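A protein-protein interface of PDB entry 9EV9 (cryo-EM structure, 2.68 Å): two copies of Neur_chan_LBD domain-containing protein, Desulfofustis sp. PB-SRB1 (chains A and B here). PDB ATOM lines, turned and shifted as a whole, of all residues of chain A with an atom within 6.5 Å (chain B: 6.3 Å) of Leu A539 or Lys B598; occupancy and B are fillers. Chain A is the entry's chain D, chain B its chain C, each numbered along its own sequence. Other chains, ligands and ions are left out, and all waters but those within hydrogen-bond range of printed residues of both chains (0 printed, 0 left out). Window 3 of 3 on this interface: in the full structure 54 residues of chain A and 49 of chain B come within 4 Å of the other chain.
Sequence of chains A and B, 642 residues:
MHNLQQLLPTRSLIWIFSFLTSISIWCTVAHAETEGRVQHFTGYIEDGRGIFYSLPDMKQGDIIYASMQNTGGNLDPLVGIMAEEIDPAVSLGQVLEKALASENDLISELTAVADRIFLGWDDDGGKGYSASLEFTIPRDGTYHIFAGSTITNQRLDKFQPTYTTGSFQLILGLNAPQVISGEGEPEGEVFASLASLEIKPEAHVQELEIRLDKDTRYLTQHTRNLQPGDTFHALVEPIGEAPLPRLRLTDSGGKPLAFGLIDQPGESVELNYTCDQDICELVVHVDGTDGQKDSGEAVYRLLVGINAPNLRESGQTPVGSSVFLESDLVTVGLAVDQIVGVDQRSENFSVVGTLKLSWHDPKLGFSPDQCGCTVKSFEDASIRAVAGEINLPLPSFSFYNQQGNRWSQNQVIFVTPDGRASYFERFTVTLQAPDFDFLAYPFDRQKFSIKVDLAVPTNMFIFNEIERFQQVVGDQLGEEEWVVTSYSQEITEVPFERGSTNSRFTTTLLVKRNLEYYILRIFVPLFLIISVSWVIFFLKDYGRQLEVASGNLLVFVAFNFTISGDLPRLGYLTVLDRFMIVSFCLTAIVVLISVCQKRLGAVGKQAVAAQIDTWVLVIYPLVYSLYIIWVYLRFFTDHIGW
Printed residues of chain B within 4 Å of Phe A538: Arg B599. Leu A539 touches one residue of chain B. Printed residues of chain B within 4 Å of Lys A540: Arg B599. Asp A541 touches none of the printed residues of chain B. Of the printed residues of chain B, Arg A544 touches Gly B543. Gln B597 touches none of the printed residues of chain A. The nearest printed residue of chain A that does not touch Leu B546 is Leu A539 (4.8 Å).
Among the printed residues, merely in contact across the chains: Lys A540 with Arg B599, Phe A538 with Arg B599, Leu A539 with Lys B598 and Val A548 with Leu B546.
The backbone carbonyl oxygen of Phe A538 is in hydrogen-bond range of the side-chain amino group of Lys A540 (3.2 Å).
Hydrophobic or aromatic side chains of chain A that line the printed part of chain B: Leu A539 and Val A548. Of the 14 printed residues of chain B, 4 touch a printed residue of chain A. Printed residues of chain B that touch a printed residue of chain A: Gly B543, Leu B546, Lys B598 and Arg B599. Hydrophobic or aromatic side chains of chain B that line the printed part of chain A: Leu B546.
O of Gly B543 sits at hydrogen-bond distance from NH1 of Arg A544, 3.5 Å away.
Position printed for both chains: 542. Of the 5 pairs that touch across the chains among the printed residues, none has its exchanged pair printed and touching as well.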
ATOM      1  N   VAL A 535       1.228  24.157  -8.561  1.00  0.00           N
ATOM      2  CA  VAL A 535       1.180  25.380  -9.354  1.00  0.00           C
ATOM      3  C   VAL A 535       2.160  25.364 -10.525  1.00  0.00           C
ATOM      4  O   VAL A 535       2.006  26.154 -11.464  1.00  0.00           O
ATOM      5  CB  VAL A 535       1.435  26.600  -8.448  1.00  0.00           C
ATOM      6  CG1 VAL A 535       2.915  26.728  -8.122  1.00  0.00           C
ATOM      7  CG2 VAL A 535       0.899  27.873  -9.084  1.00  0.00           C
ATOM      8  N   ILE A 536       3.160  24.480 -10.507  1.00  0.00           N
ATOM      9  CA  ILE A 536       4.208  24.505 -11.523  1.00  0.00           C
ATOM     10  C   ILE A 536       3.735  24.057 -12.896  1.00  0.00           C
ATOM     11  O   ILE A 536       4.481  24.200 -13.871  1.00  0.00           O
ATOM     12  CB  ILE A 536       5.405  23.638 -11.090  1.00  0.00           C
ATOM     13  CG1 ILE A 536       4.986  22.171 -10.968  1.00  0.00           C
ATOM     14  CG2 ILE A 536       5.970  24.139  -9.777  1.00  0.00           C
ATOM     15  CD1 ILE A 536       6.101  21.255 -10.515  1.00  0.00           C
ATOM     16  N   PHE A 537       2.519  23.522 -13.009  1.00  0.00           N
ATOM     17  CA  PHE A 537       2.033  23.046 -14.298  1.00  0.00           C
ATOM     18  C   PHE A 537       1.537  24.167 -15.201  1.00  0.00           C
ATOM     19  O   PHE A 537       1.186  23.896 -16.355  1.00  0.00           O
ATOM     20  CB  PHE A 537       0.928  22.007 -14.095  1.00  0.00           C
ATOM     21  CG  PHE A 537       1.445  20.637 -13.760  1.00  0.00           C
ATOM     22  CD1 PHE A 537       1.689  20.272 -12.448  1.00  0.00           C
ATOM     23  CD2 PHE A 537       1.695  19.715 -14.763  1.00  0.00           C
ATOM     24  CE1 PHE A 537       2.168  19.013 -12.143  1.00  0.00           C
ATOM     25  CE2 PHE A 537       2.174  18.458 -14.463  1.00  0.00           C
ATOM     26  CZ  PHE A 537       2.409  18.106 -13.153  1.00  0.00           C
ATOM     27  N   PHE A 538       1.490  25.410 -14.714  1.00  0.00           N
ATOM     28  CA  PHE A 538       1.165  26.532 -15.586  1.00  0.00           C
ATOM     29  C   PHE A 538       2.329  26.916 -16.489  1.00  0.00           C
ATOM     30  O   PHE A 538       2.112  27.573 -17.513  1.00  0.00           O
ATOM     31  CB  PHE A 538       0.733  27.745 -14.759  1.00  0.00           C
ATOM     32  CG  PHE A 538      -0.637  27.615 -14.163  1.00  0.00           C
ATOM     33  CD1 PHE A 538      -1.765  27.839 -14.934  1.00  0.00           C
ATOM     34  CD2 PHE A 538      -0.800  27.279 -12.831  1.00  0.00           C
ATOM     35  CE1 PHE A 538      -3.027  27.722 -14.390  1.00  0.00           C
ATOM     36  CE2 PHE A 538      -2.062  27.161 -12.280  1.00  0.00           C
ATOM     37  CZ  PHE A 538      -3.177  27.385 -13.063  1.00  0.00           C
ATOM     38  N   LEU A 539       3.550  26.527 -16.135  1.00  0.00           N
ATOM     39  CA  LEU A 539       4.714  26.850 -16.945  1.00  0.00           C
ATOM     40  C   LEU A 539       4.708  26.055 -18.246  1.00  0.00           C
ATOM     41  O   LEU A 539       4.235  24.918 -18.307  1.00  0.00           O
ATOM     42  CB  LEU A 539       6.000  26.565 -16.172  1.00  0.00           C
ATOM     43  CG  LEU A 539       6.256  27.383 -14.905  1.00  0.00           C
ATOM     44  CD1 LEU A 539       7.514  26.895 -14.207  1.00  0.00           C
ATOM     45  CD2 LEU A 539       6.362  28.864 -15.229  1.00  0.00           C
ATOM     46  N   LYS A 540       5.247  26.672 -19.298  1.00  0.00           N
ATOM     47  CA  LYS A 540       5.429  26.010 -20.581  1.00  0.00           C
ATOM     48  C   LYS A 540       6.885  25.657 -20.857  1.00  0.00           C
ATOM     49  O   LYS A 540       7.176  25.039 -21.886  1.00  0.00           O
ATOM     50  CB  LYS A 540       4.878  26.887 -21.711  1.00  0.00           C
ATOM     51  CG  LYS A 540       3.369  27.053 -21.673  1.00  0.00           C
ATOM     52  CD  LYS A 540       2.672  25.707 -21.784  1.00  0.00           C
ATOM     53  CE  LYS A 540       1.181  25.831 -21.524  1.00  0.00           C
ATOM     54  NZ  LYS A 540       0.900  26.269 -20.130  1.00  0.00           N
ATOM     55  N   ASP A 541       7.802  26.030 -19.967  1.00  0.00           N
ATOM     56  CA  ASP A 541       9.196  25.598 -20.036  1.00  0.00           C
ATOM     57  C   ASP A 541       9.342  24.408 -19.097  1.00  0.00           C
ATOM     58  O   ASP A 541       9.403  24.568 -17.876  1.00  0.00           O
ATOM     59  CB  ASP A 541      10.135  26.737 -19.660  1.00  0.00           C
ATOM     60  CG  ASP A 541      11.595  26.389 -19.881  1.00  0.00           C
ATOM     61  OD1 ASP A 541      11.876  25.337 -20.493  1.00  0.00           O
ATOM     62  OD2 ASP A 541      12.463  27.172 -19.442  1.00  0.00           O
ATOM     63  N   TYR A 542       9.404  23.205 -19.670  1.00  0.00           N
ATOM     64  CA  TYR A 542       9.289  21.992 -18.871  1.00  0.00           C
ATOM     65  C   TYR A 542      10.563  21.656 -18.107  1.00  0.00           C
ATOM     66  O   TYR A 542      10.498  20.906 -17.126  1.00  0.00           O
ATOM     67  CB  TYR A 542       8.862  20.830 -19.770  1.00  0.00           C
ATOM     68  CG  TYR A 542       7.525  21.085 -20.428  1.00  0.00           C
ATOM     69  CD1 TYR A 542       6.345  20.985 -19.701  1.00  0.00           C
ATOM     70  CD2 TYR A 542       7.443  21.450 -21.764  1.00  0.00           C
ATOM     71  CE1 TYR A 542       5.122  21.229 -20.291  1.00  0.00           C
ATOM     72  CE2 TYR A 542       6.222  21.695 -22.362  1.00  0.00           C
ATOM     73  CZ  TYR A 542       5.064  21.583 -21.620  1.00  0.00           C
ATOM     74  OH  TYR A 542       3.844  21.827 -22.206  1.00  0.00           O
ATOM     75  N   ARG A 544      12.295  23.899 -16.313  1.00  0.00           N
ATOM     76  CA  ARG A 544      12.070  24.569 -15.038  1.00  0.00           C
ATOM     77  C   ARG A 544      11.068  23.804 -14.185  1.00  0.00           C
ATOM     78  O   ARG A 544      11.248  23.672 -12.969  1.00  0.00           O
ATOM     79  CB  ARG A 544      11.588  26.001 -15.275  1.00  0.00           C
ATOM     80  CG  ARG A 544      12.652  26.940 -15.814  1.00  0.00           C
ATOM     81  CD  ARG A 544      13.695  27.259 -14.756  1.00  0.00           C
ATOM     82  NE  ARG A 544      14.672  28.232 -15.231  1.00  0.00           N
ATOM     83  CZ  ARG A 544      15.681  28.696 -14.507  1.00  0.00           C
ATOM     84  NH1 ARG A 544      15.878  28.299 -13.262  1.00  0.00           N
ATOM     85  NH2 ARG A 544      16.510  29.584 -15.046  1.00  0.00           N
ATOM     86  N   GLN A 545       9.999  23.298 -14.806  1.00  0.00           N
ATOM     87  CA  GLN A 545       9.015  22.512 -14.071  1.00  0.00           C
ATOM     88  C   GLN A 545       9.648  21.268 -13.464  1.00  0.00           C
ATOM     89  O   GLN A 545       9.410  20.949 -12.291  1.00  0.00           O
ATOM     90  CB  GLN A 545       7.857  22.135 -14.996  1.00  0.00           C
ATOM     91  CG  GLN A 545       6.909  21.095 -14.423  1.00  0.00           C
ATOM     92  CD  GLN A 545       5.756  20.784 -15.354  1.00  0.00           C
ATOM     93  OE1 GLN A 545       5.307  21.643 -16.112  1.00  0.00           O
ATOM     94  NE2 GLN A 545       5.272  19.549 -15.304  1.00  0.00           N
ATOM     95  N   VAL A 548      11.972  22.289 -10.514  1.00  0.00           N
ATOM     96  CA  VAL A 548      11.225  22.700  -9.331  1.00  0.00           C
ATOM     97  C   VAL A 548      10.554  21.499  -8.677  1.00  0.00           C
ATOM     98  O   VAL A 548      10.490  21.409  -7.448  1.00  0.00           O
ATOM     99  CB  VAL A 548      10.211  23.802  -9.689  1.00  0.00           C
ATOM    100  CG1 VAL A 548       9.331  24.124  -8.496  1.00  0.00           C
ATOM    101  CG2 VAL A 548      10.938  25.052 -10.145  1.00  0.00           C
ATOM    102  N   ASP A 613      -0.948  18.966 -19.038  1.00  0.00           N
ATOM    103  CA  ASP A 613      -0.922  19.995 -18.001  1.00  0.00           C
ATOM    104  C   ASP A 613      -2.332  20.336 -17.537  1.00  0.00           C
ATOM    105  O   ASP A 613      -2.609  20.396 -16.329  1.00  0.00           O
ATOM    106  CB  ASP A 613      -0.217  21.249 -18.521  1.00  0.00           C
ATOM    107  CG  ASP A 613       1.276  21.057 -18.689  1.00  0.00           C
ATOM    108  OD1 ASP A 613       1.866  20.271 -17.918  1.00  0.00           O
ATOM    109  OD2 ASP A 613       1.861  21.694 -19.590  1.00  0.00           O
ATOM    110  N   TYR B 542      13.551  36.183 -13.697  1.00  0.00           N
ATOM    111  CA  TYR B 542      12.689  35.494 -12.745  1.00  0.00           C
ATOM    112  C   TYR B 542      13.045  34.022 -12.573  1.00  0.00           C
ATOM    113  O   TYR B 542      12.654  33.422 -11.568  1.00  0.00           O
ATOM    114  CB  TYR B 542      11.228  35.660 -13.166  1.00  0.00           C
ATOM    115  CG  TYR B 542      10.816  37.111 -13.220  1.00  0.00           C
ATOM    116  CD1 TYR B 542      10.654  37.850 -12.053  1.00  0.00           C
ATOM    117  CD2 TYR B 542      10.609  37.754 -14.433  1.00  0.00           C
ATOM    118  CE1 TYR B 542      10.291  39.179 -12.094  1.00  0.00           C
ATOM    119  CE2 TYR B 542      10.242  39.084 -14.483  1.00  0.00           C
ATOM    120  CZ  TYR B 542      10.085  39.792 -13.309  1.00  0.00           C
ATOM    121  OH  TYR B 542       9.724  41.119 -13.349  1.00  0.00           O
ATOM    122  N   GLY B 543      13.787  33.431 -13.511  1.00  0.00           N
ATOM    123  CA  GLY B 543      14.255  32.070 -13.309  1.00  0.00           C
ATOM    124  C   GLY B 543      15.239  31.963 -12.158  1.00  0.00           C
ATOM    125  O   GLY B 543      15.135  31.062 -11.319  1.00  0.00           O
ATOM    126  N   LEU B 546      13.256  32.390  -8.928  1.00  0.00           N
ATOM    127  CA  LEU B 546      12.544  31.170  -8.561  1.00  0.00           C
ATOM    128  C   LEU B 546      13.496  30.119  -8.006  1.00  0.00           C
ATOM    129  O   LEU B 546      13.190  29.460  -7.003  1.00  0.00           O
ATOM    130  CB  LEU B 546      11.788  30.626  -9.774  1.00  0.00           C
ATOM    131  CG  LEU B 546      11.047  29.301  -9.587  1.00  0.00           C
ATOM    132  CD1 LEU B 546      10.095  29.384  -8.408  1.00  0.00           C
ATOM    133  CD2 LEU B 546      10.304  28.918 -10.856  1.00  0.00           C
ATOM    134  N   ILE B 593       4.679  33.236  -5.556  1.00  0.00           N
ATOM    135  CA  ILE B 593       4.690  34.496  -6.293  1.00  0.00           C
ATOM    136  C   ILE B 593       5.766  34.475  -7.371  1.00  0.00           C
ATOM    137  O   ILE B 593       5.590  35.042  -8.455  1.00  0.00           O
ATOM    138  CB  ILE B 593       4.872  35.680  -5.324  1.00  0.00           C
ATOM    139  CG1 ILE B 593       3.682  35.774  -4.370  1.00  0.00           C
ATOM    140  CG2 ILE B 593       5.041  36.986  -6.086  1.00  0.00           C
ATOM    141  CD1 ILE B 593       3.803  36.880  -3.349  1.00  0.00           C
ATOM    142  N   SER B 594       6.899  33.827  -7.089  1.00  0.00           N
ATOM    143  CA  SER B 594       7.951  33.711  -8.095  1.00  0.00           C
ATOM    144  C   SER B 594       7.471  32.922  -9.308  1.00  0.00           C
ATOM    145  O   SER B 594       7.744  33.303 -10.452  1.00  0.00           O
ATOM    146  CB  SER B 594       9.190  33.058  -7.487  1.00  0.00           C
ATOM    147  OG  SER B 594       9.707  33.834  -6.422  1.00  0.00           O
ATOM    148  N   VAL B 595       6.754  31.819  -9.078  1.00  0.00           N
ATOM    149  CA  VAL B 595       6.204  31.050 -10.194  1.00  0.00           C
ATOM    150  C   VAL B 595       5.216  31.896 -10.992  1.00  0.00           C
ATOM    151  O   VAL B 595       5.226  31.894 -12.233  1.00  0.00           O
ATOM    152  CB  VAL B 595       5.550  29.750  -9.687  1.00  0.00           C
ATOM    153  CG1 VAL B 595       4.886  29.010 -10.834  1.00  0.00           C
ATOM    154  CG2 VAL B 595       6.578  28.865  -9.009  1.00  0.00           C
ATOM    155  N   CYS B 596       4.344  32.624 -10.289  1.00  0.00           N
ATOM    156  CA  CYS B 596       3.368  33.467 -10.981  1.00  0.00           C
ATOM    157  C   CYS B 596       4.055  34.530 -11.831  1.00  0.00           C
ATOM    158  O   CYS B 596       3.655  34.778 -12.976  1.00  0.00           O
ATOM    159  CB  CYS B 596       2.424  34.114  -9.967  1.00  0.00           C
ATOM    160  SG  CYS B 596       1.159  35.178 -10.696  1.00  0.00           S
ATOM    161  N   GLN B 597       5.094  35.166 -11.288  1.00  0.00           N
ATOM    162  CA  GLN B 597       5.832  36.179 -12.037  1.00  0.00           C
ATOM    163  C   GLN B 597       6.553  35.572 -13.231  1.00  0.00           C
ATOM    164  O   GLN B 597       6.642  36.200 -14.293  1.00  0.00           O
ATOM    165  CB  GLN B 597       6.826  36.891 -11.123  1.00  0.00           C
ATOM    166  CG  GLN B 597       6.183  37.817 -10.118  1.00  0.00           C
ATOM    167  CD  GLN B 597       7.201  38.542  -9.272  1.00  0.00           C
ATOM    168  OE1 GLN B 597       8.156  37.944  -8.780  1.00  0.00           O
ATOM    169  NE2 GLN B 597       7.009  39.844  -9.105  1.00  0.00           N
ATOM    170  N   LYS B 598       7.097  34.363 -13.075  1.00  0.00           N
ATOM    171  CA  LYS B 598       7.735  33.694 -14.203  1.00  0.00           C
ATOM    172  C   LYS B 598       6.741  33.468 -15.333  1.00  0.00           C
ATOM    173  O   LYS B 598       7.045  33.736 -16.503  1.00  0.00           O
ATOM    174  CB  LYS B 598       8.342  32.367 -13.747  1.00  0.00           C
ATOM    175  CG  LYS B 598       9.000  31.563 -14.853  1.00  0.00           C
ATOM    176  CD  LYS B 598      10.201  32.292 -15.426  1.00  0.00           C
ATOM    177  CE  LYS B 598      10.926  31.434 -16.449  1.00  0.00           C
ATOM    178  NZ  LYS B 598      10.031  31.032 -17.568  1.00  0.00           N
ATOM    179  N   ARG B 599       5.533  33.004 -15.001  1.00  0.00           N
ATOM    180  CA  ARG B 599       4.522  32.816 -16.039  1.00  0.00           C
ATOM    181  C   ARG B 599       4.122  34.145 -16.677  1.00  0.00           C
ATOM    182  O   ARG B 599       3.981  34.237 -17.904  1.00  0.00           O
ATOM    183  CB  ARG B 599       3.298  32.101 -15.468  1.00  0.00           C
ATOM    184  CG  ARG B 599       2.223  31.810 -16.504  1.00  0.00           C
ATOM    185  CD  ARG B 599       2.809  31.123 -17.728  1.00  0.00           C
ATOM    186  NE  ARG B 599       1.844  31.016 -18.816  1.00  0.00           N
ATOM    187  CZ  ARG B 599       2.145  30.630 -20.048  1.00  0.00           C
ATOM    188  NH1 ARG B 599       3.383  30.308 -20.389  1.00  0.00           N
ATOM    189  NH2 ARG B 599       1.182  30.570 -20.964  1.00  0.00           N
ATOM    190  N   LEU B 600       3.938  35.187 -15.859  1.00  0.00           N
ATOM    191  CA  LEU B 600       3.556  36.490 -16.400  1.00  0.00           C
ATOM    192  C   LEU B 600       4.617  37.031 -17.349  1.00  0.00           C
ATOM    193  O   LEU B 600       4.292  37.591 -18.402  1.00  0.00           O
ATOM    194  CB  LEU B 600       3.298  37.482 -15.266  1.00  0.00           C
ATOM    195  CG  LEU B 600       1.889  37.501 -14.676  1.00  0.00           C
ATOM    196  CD1 LEU B 600       1.788  38.539 -13.572  1.00  0.00           C
ATOM    197  CD2 LEU B 600       0.870  37.777 -15.763  1.00  0.00           C
ATOM    198  N   GLY B 601       5.892  36.880 -16.989  1.00  0.00           N
ATOM    199  CA  GLY B 601       6.956  37.272 -17.898  1.00  0.00           C
ATOM    200  C   GLY B 601       6.979  36.432 -19.159  1.00  0.00           C
ATOM    201  O   GLY B 601       7.312  36.925 -20.238  1.00  0.00           O
ATOM    202  N   ALA B 602       6.631  35.147 -19.039  1.00  0.00           N
ATOM    203  CA  ALA B 602       6.562  34.290 -20.218  1.00  0.00           C
ATOM    204  C   ALA B 602       5.492  34.772 -21.191  1.00  0.00           C
ATOM    205  O   ALA B 602       5.702  34.768 -22.410  1.00  0.00           O
ATOM    206  CB  ALA B 602       6.299  32.844 -19.803  1.00  0.00           C
ATOM    207  N   VAL B 603       4.335  35.196 -20.673  1.00  0.00           N
ATOM    208  CA  VAL B 603       3.251  35.650 -21.548  1.00  0.00           C
ATOM    209  C   VAL B 603       3.521  37.011 -22.174  1.00  0.00           C
ATOM    210  O   VAL B 603       2.936  37.332 -23.216  1.00  0.00           O
ATOM    211  CB  VAL B 603       1.923  35.671 -20.768  1.00  0.00           C
ATOM    212  CG1 VAL B 603       0.747  35.988 -21.681  1.00  0.00           C
ATOM    213  CG2 VAL B 603       1.696  34.336 -20.081  1.00  0.00           C
